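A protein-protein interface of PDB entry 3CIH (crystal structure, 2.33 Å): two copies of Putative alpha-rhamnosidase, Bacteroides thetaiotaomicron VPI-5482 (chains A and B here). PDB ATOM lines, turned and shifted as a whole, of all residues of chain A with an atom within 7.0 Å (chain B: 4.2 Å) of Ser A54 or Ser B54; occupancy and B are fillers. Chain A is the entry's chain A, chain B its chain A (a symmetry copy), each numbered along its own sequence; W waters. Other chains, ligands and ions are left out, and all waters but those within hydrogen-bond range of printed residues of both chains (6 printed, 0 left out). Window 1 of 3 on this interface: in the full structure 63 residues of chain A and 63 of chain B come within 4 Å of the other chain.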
ATOM      1  N   ASP A  26      28.139 -12.603 -10.787  1.00  0.00           N
ATOM      2  CA  ASP A  26      28.450 -11.709  -9.677  1.00  0.00           C
ATOM      3  C   ASP A  26      28.199 -10.228  -9.949  1.00  0.00           C
ATOM      4  O   ASP A  26      27.791  -9.506  -9.043  1.00  0.00           O
ATOM      5  CB  ASP A  26      29.892 -11.917  -9.205  1.00  0.00           C
ATOM      6  CG  ASP A  26      29.998 -12.977  -8.128  1.00  0.00           C
ATOM      7  OD1 ASP A  26      28.994 -13.697  -7.919  1.00  0.00           O
ATOM      8  OD2 ASP A  26      31.077 -13.092  -7.500  1.00  0.00           O
ATOM      9  N   ILE A  29      24.343  -9.767  -9.952  1.00  0.00           N
ATOM     10  CA  ILE A  29      23.762  -9.814  -8.623  1.00  0.00           C
ATOM     11  C   ILE A  29      23.971  -8.489  -7.906  1.00  0.00           C
ATOM     12  O   ILE A  29      23.027  -7.924  -7.361  1.00  0.00           O
ATOM     13  CB  ILE A  29      24.362 -10.978  -7.797  1.00  0.00           C
ATOM     14  CG1 ILE A  29      23.821 -12.309  -8.336  1.00  0.00           C
ATOM     15  CG2 ILE A  29      24.032 -10.807  -6.327  1.00  0.00           C
ATOM     16  CD1 ILE A  29      24.405 -13.532  -7.694  1.00  0.00           C
ATOM     17  N   TRP A  30      25.201  -7.985  -7.928  1.00  0.00           N
ATOM     18  CA  TRP A  30      25.531  -6.716  -7.280  1.00  0.00           C
ATOM     19  C   TRP A  30      24.734  -5.563  -7.879  1.00  0.00           C
ATOM     20  O   TRP A  30      24.200  -4.729  -7.150  1.00  0.00           O
ATOM     21  CB  TRP A  30      27.030  -6.403  -7.415  1.00  0.00           C
ATOM     22  CG  TRP A  30      27.403  -5.038  -6.912  1.00  0.00           C
ATOM     23  CD1 TRP A  30      27.690  -4.686  -5.624  1.00  0.00           C
ATOM     24  CD2 TRP A  30      27.457  -3.827  -7.678  1.00  0.00           C
ATOM     25  NE1 TRP A  30      27.919  -3.330  -5.539  1.00  0.00           N
ATOM     26  CE2 TRP A  30      27.779  -2.780  -6.784  1.00  0.00           C
ATOM     27  CE3 TRP A  30      27.262  -3.525  -9.037  1.00  0.00           C
ATOM     28  CZ2 TRP A  30      27.907  -1.447  -7.200  1.00  0.00           C
ATOM     29  CZ3 TRP A  30      27.390  -2.198  -9.453  1.00  0.00           C
ATOM     30  CH2 TRP A  30      27.708  -1.177  -8.534  1.00  0.00           C
ATOM     31  N   ASN A  33      21.093  -5.792  -6.795  1.00  0.00           N
ATOM     32  CA  ASN A  33      20.842  -5.373  -5.429  1.00  0.00           C
ATOM     33  C   ASN A  33      20.715  -3.852  -5.442  1.00  0.00           C
ATOM     34  O   ASN A  33      19.823  -3.284  -4.806  1.00  0.00           O
ATOM     35  CB  ASN A  33      22.001  -5.780  -4.508  1.00  0.00           C
ATOM     36  CG  ASN A  33      22.114  -7.290  -4.327  1.00  0.00           C
ATOM     37  OD1 ASN A  33      21.221  -8.052  -4.708  1.00  0.00           O
ATOM     38  ND2 ASN A  33      23.215  -7.725  -3.732  1.00  0.00           N
ATOM     39  N   LYS A  51      16.004 -13.198   0.774  1.00  0.00           N
ATOM     40  CA  LYS A  51      17.433 -13.041   0.982  1.00  0.00           C
ATOM     41  C   LYS A  51      18.151 -12.325  -0.164  1.00  0.00           C
ATOM     42  O   LYS A  51      17.897 -12.589  -1.343  1.00  0.00           O
ATOM     43  CB  LYS A  51      18.048 -14.420   1.188  1.00  0.00           C
ATOM     44  CG  LYS A  51      19.545 -14.494   1.071  1.00  0.00           C
ATOM     45  CD  LYS A  51      19.975 -15.952   0.910  1.00  0.00           C
ATOM     46  CE  LYS A  51      21.489 -16.086   0.993  1.00  0.00           C
ATOM     47  NZ  LYS A  51      21.986 -17.451   0.636  1.00  0.00           N
ATOM     48  N   THR A  52      19.045 -11.411   0.200  1.00  0.00           N
ATOM     49  CA  THR A  52      19.834 -10.684  -0.783  1.00  0.00           C
ATOM     50  C   THR A  52      21.217 -11.326  -0.818  1.00  0.00           C
ATOM     51  O   THR A  52      21.875 -11.445   0.209  1.00  0.00           O
ATOM     52  CB  THR A  52      19.997  -9.188  -0.413  1.00  0.00           C
ATOM     53  OG1 THR A  52      18.738  -8.518  -0.559  1.00  0.00           O
ATOM     54  CG2 THR A  52      21.035  -8.526  -1.324  1.00  0.00           C
ATOM     55  N   ASP A  53      21.660 -11.733  -1.998  1.00  0.00           N
ATOM     56  CA  ASP A  53      22.965 -12.363  -2.112  1.00  0.00           C
ATOM     57  C   ASP A  53      24.056 -11.356  -2.442  1.00  0.00           C
ATOM     58  O   ASP A  53      23.772 -10.214  -2.779  1.00  0.00           O
ATOM     59  CB  ASP A  53      22.916 -13.491  -3.152  1.00  0.00           C
ATOM     60  CG  ASP A  53      22.192 -14.729  -2.630  1.00  0.00           C
ATOM     61  OD1 ASP A  53      22.629 -15.286  -1.598  1.00  0.00           O
ATOM     62  OD2 ASP A  53      21.192 -15.142  -3.245  1.00  0.00           O
ATOM     63  N   SER A  54      25.303 -11.792  -2.335  1.00  0.00           N
ATOM     64  CA  SER A  54      26.449 -10.932  -2.584  1.00  0.00           C
ATOM     65  C   SER A  54      27.423 -11.557  -3.571  1.00  0.00           C
ATOM     66  O   SER A  54      27.406 -12.764  -3.791  1.00  0.00           O
ATOM     67  CB  SER A  54      27.177 -10.654  -1.263  1.00  0.00           C
ATOM     68  OG  SER A  54      28.457 -10.070  -1.483  1.00  0.00           O
ATOM     69  N   HIS A  55      28.281 -10.733  -4.160  1.00  0.00           N
ATOM     70  CA  HIS A  55      29.267 -11.246  -5.094  1.00  0.00           C
ATOM     71  C   HIS A  55      30.414 -11.799  -4.261  1.00  0.00           C
ATOM     72  O   HIS A  55      30.491 -11.526  -3.071  1.00  0.00           O
ATOM     73  CB  HIS A  55      29.783 -10.132  -6.020  1.00  0.00           C
ATOM     74  CG  HIS A  55      30.415  -8.981  -5.298  1.00  0.00           C
ATOM     75  ND1 HIS A  55      29.743  -7.806  -5.040  1.00  0.00           N
ATOM     76  CD2 HIS A  55      31.651  -8.827  -4.768  1.00  0.00           C
ATOM     77  CE1 HIS A  55      30.537  -6.979  -4.382  1.00  0.00           C
ATOM     78  NE2 HIS A  55      31.702  -7.575  -4.203  1.00  0.00           N
ATOM     79  N   TYR A  56      31.287 -12.598  -4.871  1.00  0.00           N
ATOM     80  CA  TYR A  56      32.445 -13.144  -4.159  1.00  0.00           C
ATOM     81  C   TYR A  56      33.446 -11.991  -4.013  1.00  0.00           C
ATOM     82  O   TYR A  56      33.784 -11.360  -5.007  1.00  0.00           O
ATOM     83  CB  TYR A  56      33.042 -14.292  -4.974  1.00  0.00           C
ATOM     84  CG  TYR A  56      32.157 -15.518  -5.026  1.00  0.00           C
ATOM     85  CD1 TYR A  56      31.795 -16.186  -3.850  1.00  0.00           C
ATOM     86  CD2 TYR A  56      31.703 -16.033  -6.247  1.00  0.00           C
ATOM     87  CE1 TYR A  56      31.017 -17.333  -3.881  1.00  0.00           C
ATOM     88  CE2 TYR A  56      30.919 -17.181  -6.296  1.00  0.00           C
ATOM     89  CZ  TYR A  56      30.583 -17.832  -5.103  1.00  0.00           C
ATOM     90  OH  TYR A  56      29.845 -18.998  -5.120  1.00  0.00           O
ATOM     91  N   VAL A  57      33.923 -11.718  -2.795  1.00  0.00           N
ATOM     92  CA  VAL A  57      34.837 -10.587  -2.583  1.00  0.00           C
ATOM     93  C   VAL A  57      36.316 -10.764  -2.961  1.00  0.00           C
ATOM     94  O   VAL A  57      37.094  -9.803  -2.941  1.00  0.00           O
ATOM     95  CB  VAL A  57      34.737 -10.056  -1.138  1.00  0.00           C
ATOM     96  CG1 VAL A  57      33.305  -9.568  -0.865  1.00  0.00           C
ATOM     97  CG2 VAL A  57      35.135 -11.132  -0.159  1.00  0.00           C
ATOM     98  N   GLN A 113      35.198  -5.765  -1.703  1.00  0.00           N
ATOM     99  CA  GLN A 113      34.003  -5.965  -0.900  1.00  0.00           C
ATOM    100  C   GLN A 113      32.902  -4.985  -1.326  1.00  0.00           C
ATOM    101  O   GLN A 113      31.730  -5.348  -1.394  1.00  0.00           O
ATOM    102  CB  GLN A 113      34.344  -5.748   0.578  1.00  0.00           C
ATOM    103  CG  GLN A 113      33.153  -5.792   1.511  1.00  0.00           C
ATOM    104  CD  GLN A 113      32.598  -7.188   1.656  1.00  0.00           C
ATOM    105  OE1 GLN A 113      33.304  -8.105   2.088  1.00  0.00           O
ATOM    106  NE2 GLN A 113      31.328  -7.364   1.292  1.00  0.00           N
ATOM    107  N   LYS A 372      22.585 -16.766  -5.184  1.00  0.00           N
ATOM    108  CA  LYS A 372      23.710 -17.657  -4.894  1.00  0.00           C
ATOM    109  C   LYS A 372      23.289 -18.799  -3.970  1.00  0.00           C
ATOM    110  O   LYS A 372      22.169 -18.819  -3.450  1.00  0.00           O
ATOM    111  CB  LYS A 372      24.802 -16.856  -4.174  1.00  0.00           C
ATOM    112  CG  LYS A 372      26.164 -16.883  -4.781  1.00  0.00           C
ATOM    113  CD  LYS A 372      26.294 -15.808  -5.810  1.00  0.00           C
ATOM    114  CE  LYS A 372      27.734 -15.696  -6.244  1.00  0.00           C
ATOM    115  NZ  LYS A 372      28.632 -15.263  -5.135  1.00  0.00           N
ATOM    116  N   ASP B  53      34.866 -15.611   2.428  1.00  0.00           N
ATOM    117  CA  ASP B  53      33.432 -15.403   2.554  1.00  0.00           C
ATOM    118  C   ASP B  53      33.090 -13.945   2.813  1.00  0.00           C
ATOM    119  O   ASP B  53      33.966 -13.136   3.093  1.00  0.00           O
ATOM    120  CB  ASP B  53      32.863 -16.312   3.653  1.00  0.00           C
ATOM    121  CG  ASP B  53      32.770 -17.769   3.209  1.00  0.00           C
ATOM    122  OD1 ASP B  53      32.081 -18.043   2.201  1.00  0.00           O
ATOM    123  OD2 ASP B  53      33.382 -18.635   3.861  1.00  0.00           O
ATOM    124  N   SER B  54      31.809 -13.619   2.709  1.00  0.00           N
ATOM    125  CA  SER B  54      31.337 -12.256   2.894  1.00  0.00           C
ATOM    126  C   SER B  54      30.197 -12.182   3.896  1.00  0.00           C
ATOM    127  O   SER B  54      29.544 -13.182   4.181  1.00  0.00           O
ATOM    128  CB  SER B  54      30.865 -11.691   1.548  1.00  0.00           C
ATOM    129  OG  SER B  54      30.128 -10.484   1.716  1.00  0.00           O
ATOM    130  N   HIS B  55      29.950 -10.991   4.427  1.00  0.00           N
ATOM    131  CA  HIS B  55      28.860 -10.820   5.371  1.00  0.00           C
ATOM    132  C   HIS B  55      27.585 -10.686   4.550  1.00  0.00           C
ATOM    133  O   HIS B  55      27.655 -10.479   3.346  1.00  0.00           O
ATOM    134  CB  HIS B  55      29.064  -9.559   6.228  1.00  0.00           C
ATOM    135  CG  HIS B  55      29.167  -8.291   5.437  1.00  0.00           C
ATOM    136  ND1 HIS B  55      30.373  -7.703   5.127  1.00  0.00           N
ATOM    137  CD2 HIS B  55      28.215  -7.505   4.879  1.00  0.00           C
ATOM    138  CE1 HIS B  55      30.161  -6.610   4.413  1.00  0.00           C
ATOM    139  NE2 HIS B  55      28.859  -6.468   4.247  1.00  0.00           N
ATOM    140  N   TYR B  56      26.426 -10.832   5.187  1.00  0.00           N
ATOM    141  CA  TYR B  56      25.148 -10.680   4.487  1.00  0.00           C
ATOM    142  C   TYR B  56      24.953  -9.175   4.264  1.00  0.00           C
ATOM    143  O   TYR B  56      25.040  -8.411   5.218  1.00  0.00           O
ATOM    144  CB  TYR B  56      24.027 -11.258   5.352  1.00  0.00           C
ATOM    145  CG  TYR B  56      24.084 -12.765   5.483  1.00  0.00           C
ATOM    146  CD1 TYR B  56      23.995 -13.582   4.350  1.00  0.00           C
ATOM    147  CD2 TYR B  56      24.195 -13.380   6.736  1.00  0.00           C
ATOM    148  CE1 TYR B  56      24.006 -14.965   4.454  1.00  0.00           C
ATOM    149  CE2 TYR B  56      24.210 -14.765   6.859  1.00  0.00           C
ATOM    150  CZ  TYR B  56      24.109 -15.555   5.708  1.00  0.00           C
ATOM    151  OH  TYR B  56      24.076 -16.932   5.799  1.00  0.00           O
ATOM    152  N   VAL B  57      24.689  -8.748   3.026  1.00  0.00           N
ATOM    153  CA  VAL B  57      24.554  -7.313   2.740  1.00  0.00           C
ATOM    154  C   VAL B  57      23.231  -6.619   3.102  1.00  0.00           C
ATOM    155  O   VAL B  57      23.117  -5.390   3.019  1.00  0.00           O
ATOM    156  CB  VAL B  57      24.908  -7.005   1.270  1.00  0.00           C
ATOM    157  CG1 VAL B  57      26.366  -7.409   0.994  1.00  0.00           C
ATOM    158  CG2 VAL B  57      23.965  -7.728   0.343  1.00  0.00           C
ATOM    159  N   GLN B 113      26.917  -3.157   1.599  1.00  0.00           N
ATOM    160  CA  GLN B 113      27.786  -4.029   0.827  1.00  0.00           C
ATOM    161  C   GLN B 113      29.253  -3.804   1.219  1.00  0.00           C
ATOM    162  O   GLN B 113      30.027  -4.753   1.324  1.00  0.00           O
ATOM    163  CB  GLN B 113      27.599  -3.738  -0.666  1.00  0.00           C
ATOM    164  CG  GLN B 113      28.550  -4.485  -1.576  1.00  0.00           C
ATOM    165  CD  GLN B 113      28.235  -5.959  -1.637  1.00  0.00           C
ATOM    166  OE1 GLN B 113      27.131  -6.352  -2.031  1.00  0.00           O
ATOM    167  NE2 GLN B 113      29.199  -6.791  -1.244  1.00  0.00           N
ATOM    168  N   LYS B 372      31.354 -19.106   5.861  1.00  0.00           N
ATOM    169  CA  LYS B 372      29.919 -19.237   5.600  1.00  0.00           C
ATOM    170  C   LYS B 372      29.619 -20.467   4.745  1.00  0.00           C
ATOM    171  O   LYS B 372      30.532 -21.133   4.245  1.00  0.00           O
ATOM    172  CB  LYS B 372      29.444 -18.004   4.821  1.00  0.00           C
ATOM    173  CG  LYS B 372      28.306 -17.238   5.407  1.00  0.00           C
ATOM    174  CD  LYS B 372      28.811 -16.219   6.375  1.00  0.00           C
ATOM    175  CE  LYS B 372      27.682 -15.303   6.779  1.00  0.00           C
ATOM    176  NZ  LYS B 372      27.158 -14.504   5.635  1.00  0.00           N
HETATM  177  O   HOH W   1      27.091  -7.995  -4.411  1.00  0.00           O
HETATM  178  O   HOH W   2      21.884 -10.569   2.808  1.00  0.00           O
HETATM  179  O   HOH W   3      22.446 -18.754   3.707  1.00  0.00           O
HETATM  180  O   HOH W   4      24.528 -10.970   1.034  1.00  0.00           O
HETATM  181  O   HOH W   5      24.638  -5.285  -2.518  1.00  0.00           O
HETATM  182  O   HOH W   6      32.463  -9.366   4.552  1.00  0.00           O
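OG of Ser A54 is in hydrogen-bond range of NE2 of Gln B113 (3.4 Å). OG of Ser B54 sits at hydrogen-bond distance from NE2 of Gln A113, at 3.4 Å. NE2 of Gln B113 is in hydrogen-bond range of O of Gln A113, 2.9 Å away.
Trp A30 touches Gln B113 (CD1 to OE1, 3.9997 Å). CG2 of Thr A52 touches CG2 of Val B57, at 3.5 Å. O of Asp A53 touches CG2 of Val B57, at 3.996 Å. OG of Ser A54 touches OG of Ser B54, 3.6 Å away. Gln B113 touches His A55 (NE2 to CE1, 3.4 Å). Asp B53 touches Val A57 (O to CG2, 3.99 Å). His B55 touches Gln A113 (CE1 to NE2, 3.4 Å).
Hydrophobic or aromatic side chains of chain A within 4 Å of the printed part of chain B: Trp A30, His A55 and Val A57. Of the 7 printed residues of chain B, 5 touch a printed residue of chain A. Hydrophobic or aromatic side chains of chain B that line the printed part of chain A: His B55 and Val B57. Along chain B the printed residues that touch a printed residue of chain A span positions 53 to 113. Among the printed residues, 10 pairs touch across the chains. Among the printed residues, no Asp or Glu carboxylate lies within 4 Å of a Lys or Arg side-chain nitrogen of the other chain.
Asp A53 touches Val B57, and with the chains exchanged Val A57 touches Asp B53. Ser A54 touches Gln B113, and with the chains exchanged Gln A113 touches Ser B54. His A55 touches Gln B113, and with the chains exchanged Gln A113 touches His B55. Gln A113 touches its own counterpart, Gln B113. 7 positions are printed for both chains.
The side-chain carboxylate (OD2) of Asp A53 sits at hydrogen-bond distance from the backbone NH (N) of Lys A372 (2.9 Å). NZ of Lys B372 sits at hydrogen-bond distance from O of Ser B54 (3.1 Å). The side-chain amino group (NZ) of Lys A372 sits at hydrogen-bond distance from the backbone carbonyl oxygen (O) of Ser A54, at 3.1 Å. The side-chain amino group (NZ) of Lys A51 lies within salt-bridge range of the side-chain carboxylate (OD1) of Asp A53 (3.2 Å). OD2 of Asp B53 sits at hydrogen-bond distance from N of Lys B372 (2.9 Å). ND2 of Asn A33 is in hydrogen-bond range of O of Asp A53 (2.7 Å).
Of the printed residues of chain B, Ser A54 touches Ser B54 (3.6 Å) and Gln B113 (3.4 Å). Of chain A, only Ser A54 (3.6 Å) and Gln A113 (3.4 Å) come within 4 Å of Ser B54. Of the printed residues of chain B, Gln A113 touches Ser B54 (3.4 Å), His B55 (3.4 Å) and Gln B113 (2.9 Å). Of the printed residues of chain A, His B55 touches Gln A113 (3.4 Å). Lys B372 touches none of the printed residues of chain A. Asn A33 touches none of the printed residues of chain B. The nearest residue of chain A that does not touch Ser B54 is Val A57 (4.04 Å).
Water W1 lies within hydrogen-bond range of a ring nitrogen (ND1) of His A55 (2.7 Å) and the side-chain amide oxygen (OE1) of Gln B113 (2.9 Å). Water W6 bridges a ring nitrogen (ND1) of His B55 (2.7 Å) and the side-chain amide oxygen of Gln A113 (2.9 Å). Water W2 bridges the backbone carbonyl oxygen (O) of Thr A52 and the backbone NH (N) of Val B57. Water W5 lies within hydrogen-bond range of OE1 of Gln B113 (2.8 Å) and ND2 of Asn A33 (3.1 Å). Water W4 lies within hydrogen-bond range of the backbone carbonyl oxygen of Thr A52 (2.8 Å) and the backbone NH of Val B57 (3.0 Å). Water W3 lies within hydrogen-bond range of OH of Tyr B56 and NZ of Lys A51.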
